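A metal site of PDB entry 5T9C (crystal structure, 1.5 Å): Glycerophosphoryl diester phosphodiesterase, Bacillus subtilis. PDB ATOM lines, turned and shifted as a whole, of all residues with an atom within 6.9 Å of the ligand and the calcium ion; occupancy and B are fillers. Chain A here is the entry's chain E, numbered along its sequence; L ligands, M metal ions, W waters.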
ATOM      1  N   HIS A  18      19.784  18.938   6.673  1.00  0.00           N
ATOM      2  CA  HIS A  18      18.357  19.175   6.901  1.00  0.00           C
ATOM      3  C   HIS A  18      18.114  20.235   7.967  1.00  0.00           C
ATOM      4  O   HIS A  18      18.295  19.981   9.157  1.00  0.00           O
ATOM      5  CB  HIS A  18      17.728  17.848   7.316  1.00  0.00           C
ATOM      6  CG  HIS A  18      16.243  17.887   7.498  1.00  0.00           C
ATOM      7  ND1 HIS A  18      15.641  17.582   8.704  1.00  0.00           N
ATOM      8  CD2 HIS A  18      15.238  18.182   6.631  1.00  0.00           C
ATOM      9  CE1 HIS A  18      14.321  17.675   8.562  1.00  0.00           C
ATOM     10  NE2 HIS A  18      14.062  18.041   7.321  1.00  0.00           N
ATOM     11  N   ARG A  19      17.686  21.431   7.534  1.00  0.00           N
ATOM     12  CA  ARG A  19      17.496  22.578   8.433  1.00  0.00           C
ATOM     13  C   ARG A  19      18.807  22.938   9.129  1.00  0.00           C
ATOM     14  O   ARG A  19      18.818  23.431  10.253  1.00  0.00           O
ATOM     15  CB  ARG A  19      16.379  22.292   9.445  1.00  0.00           C
ATOM     16  CG  ARG A  19      15.163  21.550   8.831  1.00  0.00           C
ATOM     17  CD  ARG A  19      13.977  21.419   9.777  1.00  0.00           C
ATOM     18  NE  ARG A  19      12.971  20.537   9.196  1.00  0.00           N
ATOM     19  CZ  ARG A  19      11.959  19.985   9.870  1.00  0.00           C
ATOM     20  NH1 ARG A  19      11.789  20.247  11.157  1.00  0.00           N
ATOM     21  NH2 ARG A  19      11.124  19.153   9.263  1.00  0.00           N
ATOM     22  N   HIS A  28      17.144  25.742  11.418  1.00  0.00           N
ATOM     23  CA  HIS A  28      16.913  26.986  10.675  1.00  0.00           C
ATOM     24  C   HIS A  28      17.340  28.219  11.462  1.00  0.00           C
ATOM     25  O   HIS A  28      16.623  29.228  11.489  1.00  0.00           O
ATOM     26  CB  HIS A  28      15.443  27.094  10.282  1.00  0.00           C
ATOM     27  CG  HIS A  28      15.009  26.082   9.258  1.00  0.00           C
ATOM     28  ND1 HIS A  28      15.804  25.714   8.192  1.00  0.00           N
ATOM     29  CD2 HIS A  28      13.859  25.391   9.132  1.00  0.00           C
ATOM     30  CE1 HIS A  28      15.147  24.845   7.445  1.00  0.00           C
ATOM     31  NE2 HIS A  28      13.963  24.624   7.992  1.00  0.00           N
ATOM     32  N   GLU A  45      20.080  23.352   4.045  1.00  0.00           N
ATOM     33  CA  GLU A  45      18.699  23.221   3.598  1.00  0.00           C
ATOM     34  C   GLU A  45      17.767  24.185   4.322  1.00  0.00           C
ATOM     35  O   GLU A  45      17.749  24.249   5.551  1.00  0.00           O
ATOM     36  CB  GLU A  45      18.235  21.762   3.797  1.00  0.00           C
ATOM     37  CG  GLU A  45      16.959  21.426   3.035  1.00  0.00           C
ATOM     38  CD  GLU A  45      15.734  21.297   3.922  1.00  0.00           C
ATOM     39  OE1 GLU A  45      15.849  21.303   5.171  1.00  0.00           O
ATOM     40  OE2 GLU A  45      14.621  21.188   3.362  1.00  0.00           O
ATOM     41  N   LEU A  46      17.010  24.950   3.531  1.00  0.00           N
ATOM     42  CA  LEU A  46      16.123  25.981   4.032  1.00  0.00           C
ATOM     43  C   LEU A  46      14.676  25.662   3.689  1.00  0.00           C
ATOM     44  O   LEU A  46      14.418  25.192   2.590  1.00  0.00           O
ATOM     45  CB  LEU A  46      16.473  27.340   3.420  1.00  0.00           C
ATOM     46  CG  LEU A  46      17.720  28.093   3.892  1.00  0.00           C
ATOM     47  CD1 LEU A  46      19.025  27.307   3.762  1.00  0.00           C
ATOM     48  CD2 LEU A  46      17.790  29.361   3.039  1.00  0.00           C
ATOM     49  N   ASP A  47      13.758  25.954   4.608  1.00  0.00           N
ATOM     50  CA  ASP A  47      12.315  25.932   4.337  1.00  0.00           C
ATOM     51  C   ASP A  47      11.827  27.373   4.373  1.00  0.00           C
ATOM     52  O   ASP A  47      12.140  28.083   5.334  1.00  0.00           O
ATOM     53  CB  ASP A  47      11.544  25.109   5.363  1.00  0.00           C
ATOM     54  CG  ASP A  47      11.937  23.647   5.400  1.00  0.00           C
ATOM     55  OD1 ASP A  47      12.009  22.979   4.328  1.00  0.00           O
ATOM     56  OD2 ASP A  47      12.129  23.157   6.525  1.00  0.00           O
ATOM     57  N   HIS A  60      10.331  26.010   9.155  1.00  0.00           N
ATOM     58  CA  HIS A  60       9.684  24.825   8.587  1.00  0.00           C
ATOM     59  C   HIS A  60       8.165  24.911   8.605  1.00  0.00           C
ATOM     60  O   HIS A  60       7.510  24.653   7.592  1.00  0.00           O
ATOM     61  CB  HIS A  60      10.108  23.551   9.305  1.00  0.00           C
ATOM     62  CG  HIS A  60       9.370  22.350   8.822  1.00  0.00           C
ATOM     63  ND1 HIS A  60       8.187  21.929   9.392  1.00  0.00           N
ATOM     64  CD2 HIS A  60       9.604  21.525   7.778  1.00  0.00           C
ATOM     65  CE1 HIS A  60       7.742  20.864   8.745  1.00  0.00           C
ATOM     66  NE2 HIS A  60       8.588  20.604   7.758  1.00  0.00           N
ATOM     67  N   TYR A 125      19.853  24.589  -0.580  1.00  0.00           N
ATOM     68  CA  TYR A 125      18.796  23.658  -0.977  1.00  0.00           C
ATOM     69  C   TYR A 125      17.513  24.215  -0.405  1.00  0.00           C
ATOM     70  O   TYR A 125      17.270  24.093   0.785  1.00  0.00           O
ATOM     71  CB  TYR A 125      19.112  22.264  -0.425  1.00  0.00           C
ATOM     72  CG  TYR A 125      18.666  21.086  -1.262  1.00  0.00           C
ATOM     73  CD1 TYR A 125      19.573  20.106  -1.654  1.00  0.00           C
ATOM     74  CD2 TYR A 125      17.342  20.944  -1.661  1.00  0.00           C
ATOM     75  CE1 TYR A 125      19.184  19.003  -2.381  1.00  0.00           C
ATOM     76  CE2 TYR A 125      16.936  19.841  -2.407  1.00  0.00           C
ATOM     77  CZ  TYR A 125      17.858  18.877  -2.762  1.00  0.00           C
ATOM     78  OH  TYR A 125      17.445  17.784  -3.502  1.00  0.00           O
ATOM     79  N   GLU A 127      13.471  25.085  -0.002  1.00  0.00           N
ATOM     80  CA  GLU A 127      12.100  24.623  -0.213  1.00  0.00           C
ATOM     81  C   GLU A 127      11.062  25.725  -0.137  1.00  0.00           C
ATOM     82  O   GLU A 127      11.057  26.536   0.785  1.00  0.00           O
ATOM     83  CB  GLU A 127      11.742  23.541   0.808  1.00  0.00           C
ATOM     84  CG  GLU A 127      10.369  22.911   0.515  1.00  0.00           C
ATOM     85  CD  GLU A 127      10.042  21.755   1.441  1.00  0.00           C
ATOM     86  OE1 GLU A 127      10.977  21.215   2.091  1.00  0.00           O
ATOM     87  OE2 GLU A 127       8.851  21.388   1.485  1.00  0.00           O
ATOM     88  N   LYS A 129       7.571  26.356   0.883  1.00  0.00           N
ATOM     89  CA  LYS A 129       6.496  25.776   1.678  1.00  0.00           C
ATOM     90  C   LYS A 129       5.177  26.450   1.384  1.00  0.00           C
ATOM     91  O   LYS A 129       5.116  27.667   1.262  1.00  0.00           O
ATOM     92  CB  LYS A 129       6.783  25.905   3.175  1.00  0.00           C
ATOM     93  CG  LYS A 129       7.916  25.025   3.680  1.00  0.00           C
ATOM     94  CD  LYS A 129       7.535  23.541   3.632  1.00  0.00           C
ATOM     95  CE  LYS A 129       8.598  22.727   4.360  1.00  0.00           C
ATOM     96  NZ  LYS A 129       8.364  21.249   4.208  1.00  0.00           N
ATOM     97  N   GLN A 163      13.436  23.168  -4.189  1.00  0.00           N
ATOM     98  CA  GLN A 163      12.685  21.943  -3.951  1.00  0.00           C
ATOM     99  C   GLN A 163      11.306  22.295  -3.438  1.00  0.00           C
ATOM    100  O   GLN A 163      11.101  23.375  -2.885  1.00  0.00           O
ATOM    101  CB  GLN A 163      13.417  21.064  -2.932  1.00  0.00           C
ATOM    102  CG  GLN A 163      13.863  21.882  -1.728  1.00  0.00           C
ATOM    103  CD  GLN A 163      14.141  21.060  -0.489  1.00  0.00           C
ATOM    104  OE1 GLN A 163      13.889  19.843  -0.453  1.00  0.00           O
ATOM    105  NE2 GLN A 163      14.684  21.715   0.542  1.00  0.00           N
ATOM    106  N   SER A 164      10.346  21.389  -3.613  1.00  0.00           N
ATOM    107  CA  SER A 164       9.003  21.632  -3.101  1.00  0.00           C
ATOM    108  C   SER A 164       8.192  20.344  -3.216  1.00  0.00           C
ATOM    109  O   SER A 164       8.447  19.524  -4.088  1.00  0.00           O
ATOM    110  CB  SER A 164       8.304  22.750  -3.883  1.00  0.00           C
ATOM    111  OG  SER A 164       7.105  23.176  -3.255  1.00  0.00           O
ATOM    112  N   PHE A 165       7.202  20.213  -2.342  1.00  0.00           N
ATOM    113  CA  PHE A 165       6.142  19.236  -2.568  1.00  0.00           C
ATOM    114  C   PHE A 165       5.190  19.696  -3.671  1.00  0.00           C
ATOM    115  O   PHE A 165       4.523  18.868  -4.308  1.00  0.00           O
ATOM    116  CB  PHE A 165       5.378  18.971  -1.272  1.00  0.00           C
ATOM    117  CG  PHE A 165       6.146  18.122  -0.298  1.00  0.00           C
ATOM    118  CD1 PHE A 165       6.155  16.745  -0.423  1.00  0.00           C
ATOM    119  CD2 PHE A 165       6.869  18.706   0.731  1.00  0.00           C
ATOM    120  CE1 PHE A 165       6.884  15.961   0.480  1.00  0.00           C
ATOM    121  CE2 PHE A 165       7.583  17.936   1.625  1.00  0.00           C
ATOM    122  CZ  PHE A 165       7.601  16.563   1.504  1.00  0.00           C
ATOM    123  N   LEU A 185       9.782  16.919  -4.335  1.00  0.00           N
ATOM    124  CA  LEU A 185       9.622  16.181  -3.094  1.00  0.00           C
ATOM    125  C   LEU A 185       8.377  15.306  -3.140  1.00  0.00           C
ATOM    126  O   LEU A 185       7.340  15.666  -3.725  1.00  0.00           O
ATOM    127  CB  LEU A 185       9.558  17.131  -1.903  1.00  0.00           C
ATOM    128  CG  LEU A 185      10.771  18.057  -1.726  1.00  0.00           C
ATOM    129  CD1 LEU A 185      10.532  18.967  -0.544  1.00  0.00           C
ATOM    130  CD2 LEU A 185      12.034  17.215  -1.524  1.00  0.00           C
ATOM    131  N   GLY A 210      13.009  13.730  -4.341  1.00  0.00           N
ATOM    132  CA  GLY A 210      13.306  13.685  -2.920  1.00  0.00           C
ATOM    133  C   GLY A 210      12.166  13.011  -2.180  1.00  0.00           C
ATOM    134  O   GLY A 210      11.273  13.682  -1.665  1.00  0.00           O
ATOM    135  N   HIS A 232      17.478  12.005  -3.669  1.00  0.00           N
ATOM    136  CA  HIS A 232      17.836  12.552  -2.356  1.00  0.00           C
ATOM    137  C   HIS A 232      16.737  12.282  -1.350  1.00  0.00           C
ATOM    138  O   HIS A 232      15.869  13.131  -1.140  1.00  0.00           O
ATOM    139  CB  HIS A 232      18.059  14.076  -2.435  1.00  0.00           C
ATOM    140  CG  HIS A 232      19.160  14.484  -3.355  1.00  0.00           C
ATOM    141  ND1 HIS A 232      19.256  15.767  -3.861  1.00  0.00           N
ATOM    142  CD2 HIS A 232      20.229  13.804  -3.840  1.00  0.00           C
ATOM    143  CE1 HIS A 232      20.328  15.846  -4.638  1.00  0.00           C
ATOM    144  NE2 HIS A 232      20.932  14.678  -4.630  1.00  0.00           N
ATOM    145  N   PRO A 233      16.765  11.113  -0.714  1.00  0.00           N
ATOM    146  CA  PRO A 233      15.671  10.825   0.231  1.00  0.00           C
ATOM    147  C   PRO A 233      15.826  11.608   1.530  1.00  0.00           C
ATOM    148  O   PRO A 233      16.954  11.999   1.883  1.00  0.00           O
ATOM    149  CB  PRO A 233      15.789   9.312   0.470  1.00  0.00           C
ATOM    150  CG  PRO A 233      17.152   8.943   0.064  1.00  0.00           C
ATOM    151  CD  PRO A 233      17.618   9.938  -0.964  1.00  0.00           C
ATOM    152  N   TYR A 234      14.704  11.846   2.211  1.00  0.00           N
ATOM    153  CA  TYR A 234      14.658  12.555   3.494  1.00  0.00           C
ATOM    154  C   TYR A 234      13.888  11.677   4.487  1.00  0.00           C
ATOM    155  O   TYR A 234      13.125  10.804   4.059  1.00  0.00           O
ATOM    156  CB  TYR A 234      13.957  13.929   3.368  1.00  0.00           C
ATOM    157  CG  TYR A 234      12.475  13.794   3.055  1.00  0.00           C
ATOM    158  CD1 TYR A 234      11.544  13.627   4.069  1.00  0.00           C
ATOM    159  CD2 TYR A 234      12.019  13.806   1.739  1.00  0.00           C
ATOM    160  CE1 TYR A 234      10.187  13.468   3.791  1.00  0.00           C
ATOM    161  CE2 TYR A 234      10.672  13.659   1.452  1.00  0.00           C
ATOM    162  CZ  TYR A 234       9.753  13.479   2.483  1.00  0.00           C
ATOM    163  OH  TYR A 234       8.404  13.324   2.208  1.00  0.00           O
ATOM    164  N   THR A 235      14.063  11.865   5.796  1.00  0.00           N
ATOM    165  CA  THR A 235      15.233  12.496   6.421  1.00  0.00           C
ATOM    166  C   THR A 235      15.972  11.355   7.115  1.00  0.00           C
ATOM    167  O   THR A 235      15.399  10.663   7.960  1.00  0.00           O
ATOM    168  CB  THR A 235      14.830  13.573   7.430  1.00  0.00           C
ATOM    169  OG1 THR A 235      14.190  14.648   6.733  1.00  0.00           O
ATOM    170  CG2 THR A 235      16.070  14.119   8.164  1.00  0.00           C
ATOM    171  N   PHE A 254      18.982  13.996   2.717  1.00  0.00           N
ATOM    172  CA  PHE A 254      18.730  15.022   3.720  1.00  0.00           C
ATOM    173  C   PHE A 254      18.955  14.385   5.080  1.00  0.00           C
ATOM    174  O   PHE A 254      18.361  13.330   5.376  1.00  0.00           O
ATOM    175  CB  PHE A 254      17.295  15.582   3.648  1.00  0.00           C
ATOM    176  CG  PHE A 254      16.919  16.216   2.336  1.00  0.00           C
ATOM    177  CD1 PHE A 254      16.497  15.447   1.265  1.00  0.00           C
ATOM    178  CD2 PHE A 254      16.939  17.606   2.186  1.00  0.00           C
ATOM    179  CE1 PHE A 254      16.126  16.032   0.072  1.00  0.00           C
ATOM    180  CE2 PHE A 254      16.564  18.200   0.990  1.00  0.00           C
ATOM    181  CZ  PHE A 254      16.152  17.404  -0.073  1.00  0.00           C
HETATM  182  O1  LIG L   1      13.011  18.991   1.848  1.00  0.00           O
HETATM  183  C1  LIG L   1      13.128  17.594   2.111  1.00  0.00           C
HETATM  184  C2  LIG L   1      12.469  17.343   3.448  1.00  0.00           C
HETATM  185  O2  LIG L   1      12.960  18.300   4.373  1.00  0.00           O
HETATM  186  C3  LIG L   1      10.956  17.406   3.275  1.00  0.00           C
HETATM  187  O3  LIG L   1      10.305  17.331   4.530  1.00  0.00           O
HETATM  188  O4  LIG L   1       8.892  18.433   6.302  1.00  0.00           O
HETATM  189  O5  LIG L   1      11.353  18.154   6.660  1.00  0.00           O
HETATM  190  O6  LIG L   1      10.505  19.786   4.963  1.00  0.00           O
HETATM  191  P1  LIG L   1      10.264  18.456   5.658  1.00  0.00           P
HETATM  192 CA    CA M   1      12.407  20.632   3.806  1.00  0.00          CA
HETATM  193  O   HOH W   1      13.369  20.835   6.158  1.00  0.00           O
HETATM  194  O   HOH W   2      11.695  15.393   7.531  1.00  0.00           O
HETATM  195  O   HOH W   3       7.209  16.199   6.143  1.00  0.00           O
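An oxygen (O1) of the ligand lies close to the side-chain amide oxygen (OE1) of Gln 163 (2.6 Å). A ring nitrogen (NE2) of His 60 sits at hydrogen-bond distance from an oxygen (O4) of the ligand, at 2.6 Å. The side-chain amino group (NZ) of Lys 129 is in salt-bridge range of an oxygen (O4) of the ligand, 3.5 Å away. A ring nitrogen (NE2) of His 18 sits at hydrogen-bond distance from an oxygen (O5) of the ligand (2.8 Å). NH2 of Arg 19 is in salt-bridge range of O5 of the ligand (2.8 Å).
The side-chain carboxylate (OE2) of Glu 127 is in salt-bridge range of the side-chain amino group (NZ) of Lys 129. The backbone NH (N) of Glu 127 is in hydrogen-bond range of the backbone carbonyl oxygen (O) of Leu 46 (2.8 Å). NE2 of Gln 163 lies close to OE2 of Glu 45. The side-chain carboxylate of Glu 45 sits at hydrogen-bond distance from the backbone NH of Arg 19 (3.0 Å). A ring nitrogen (NE2) of His 28 lies within hydrogen-bond range of the side-chain carboxylate of Asp 47, 2.8 Å away. NE2 of His 60 lies close to NH2 of Arg 19, 3.3 Å away. O of Arg 19 lies within hydrogen-bond range of N of His 28, at 3.1 Å. N of Phe 254 sits at hydrogen-bond distance from O of Pro 233, 3.0 Å away.
Residues that only touch the ligand: Leu 185 (3.4 Å), Tyr 234 (3.6 Å), Phe 254 (3.7 Å) and Phe 165 (3.8 Å). Hydrophobic or aromatic side chains that line the ligand: His 18, His 60, Phe 165, Leu 185, Tyr 234 and Phe 254.
Within 4 Å of the calcium ion: Glu 45, Asp 47 and Glu 127.
The calcium ion is bound by the side-chain carboxylate of Glu 127 (2.3 Å), the side-chain carboxylate of Glu 45 (2.3 Å), an oxygen (O6) of the ligand (2.4 Å), the side-chain carboxylate of Asp 47 (2.4 Å), an oxygen (O2) of the ligand (2.5 Å), water W1 (2.5 Å) and an oxygen (O1) of the ligand (2.6 Å).
Water W1 lies within hydrogen-bond range of OD2 of Asp 47, OE1 of Glu 45, NE of Arg 19, NE2 of His 18 and O5 of the ligand. Water W2 bridges OG1 of Thr 235 (2.7 Å) and O5 of the ligand (2.9 Å).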
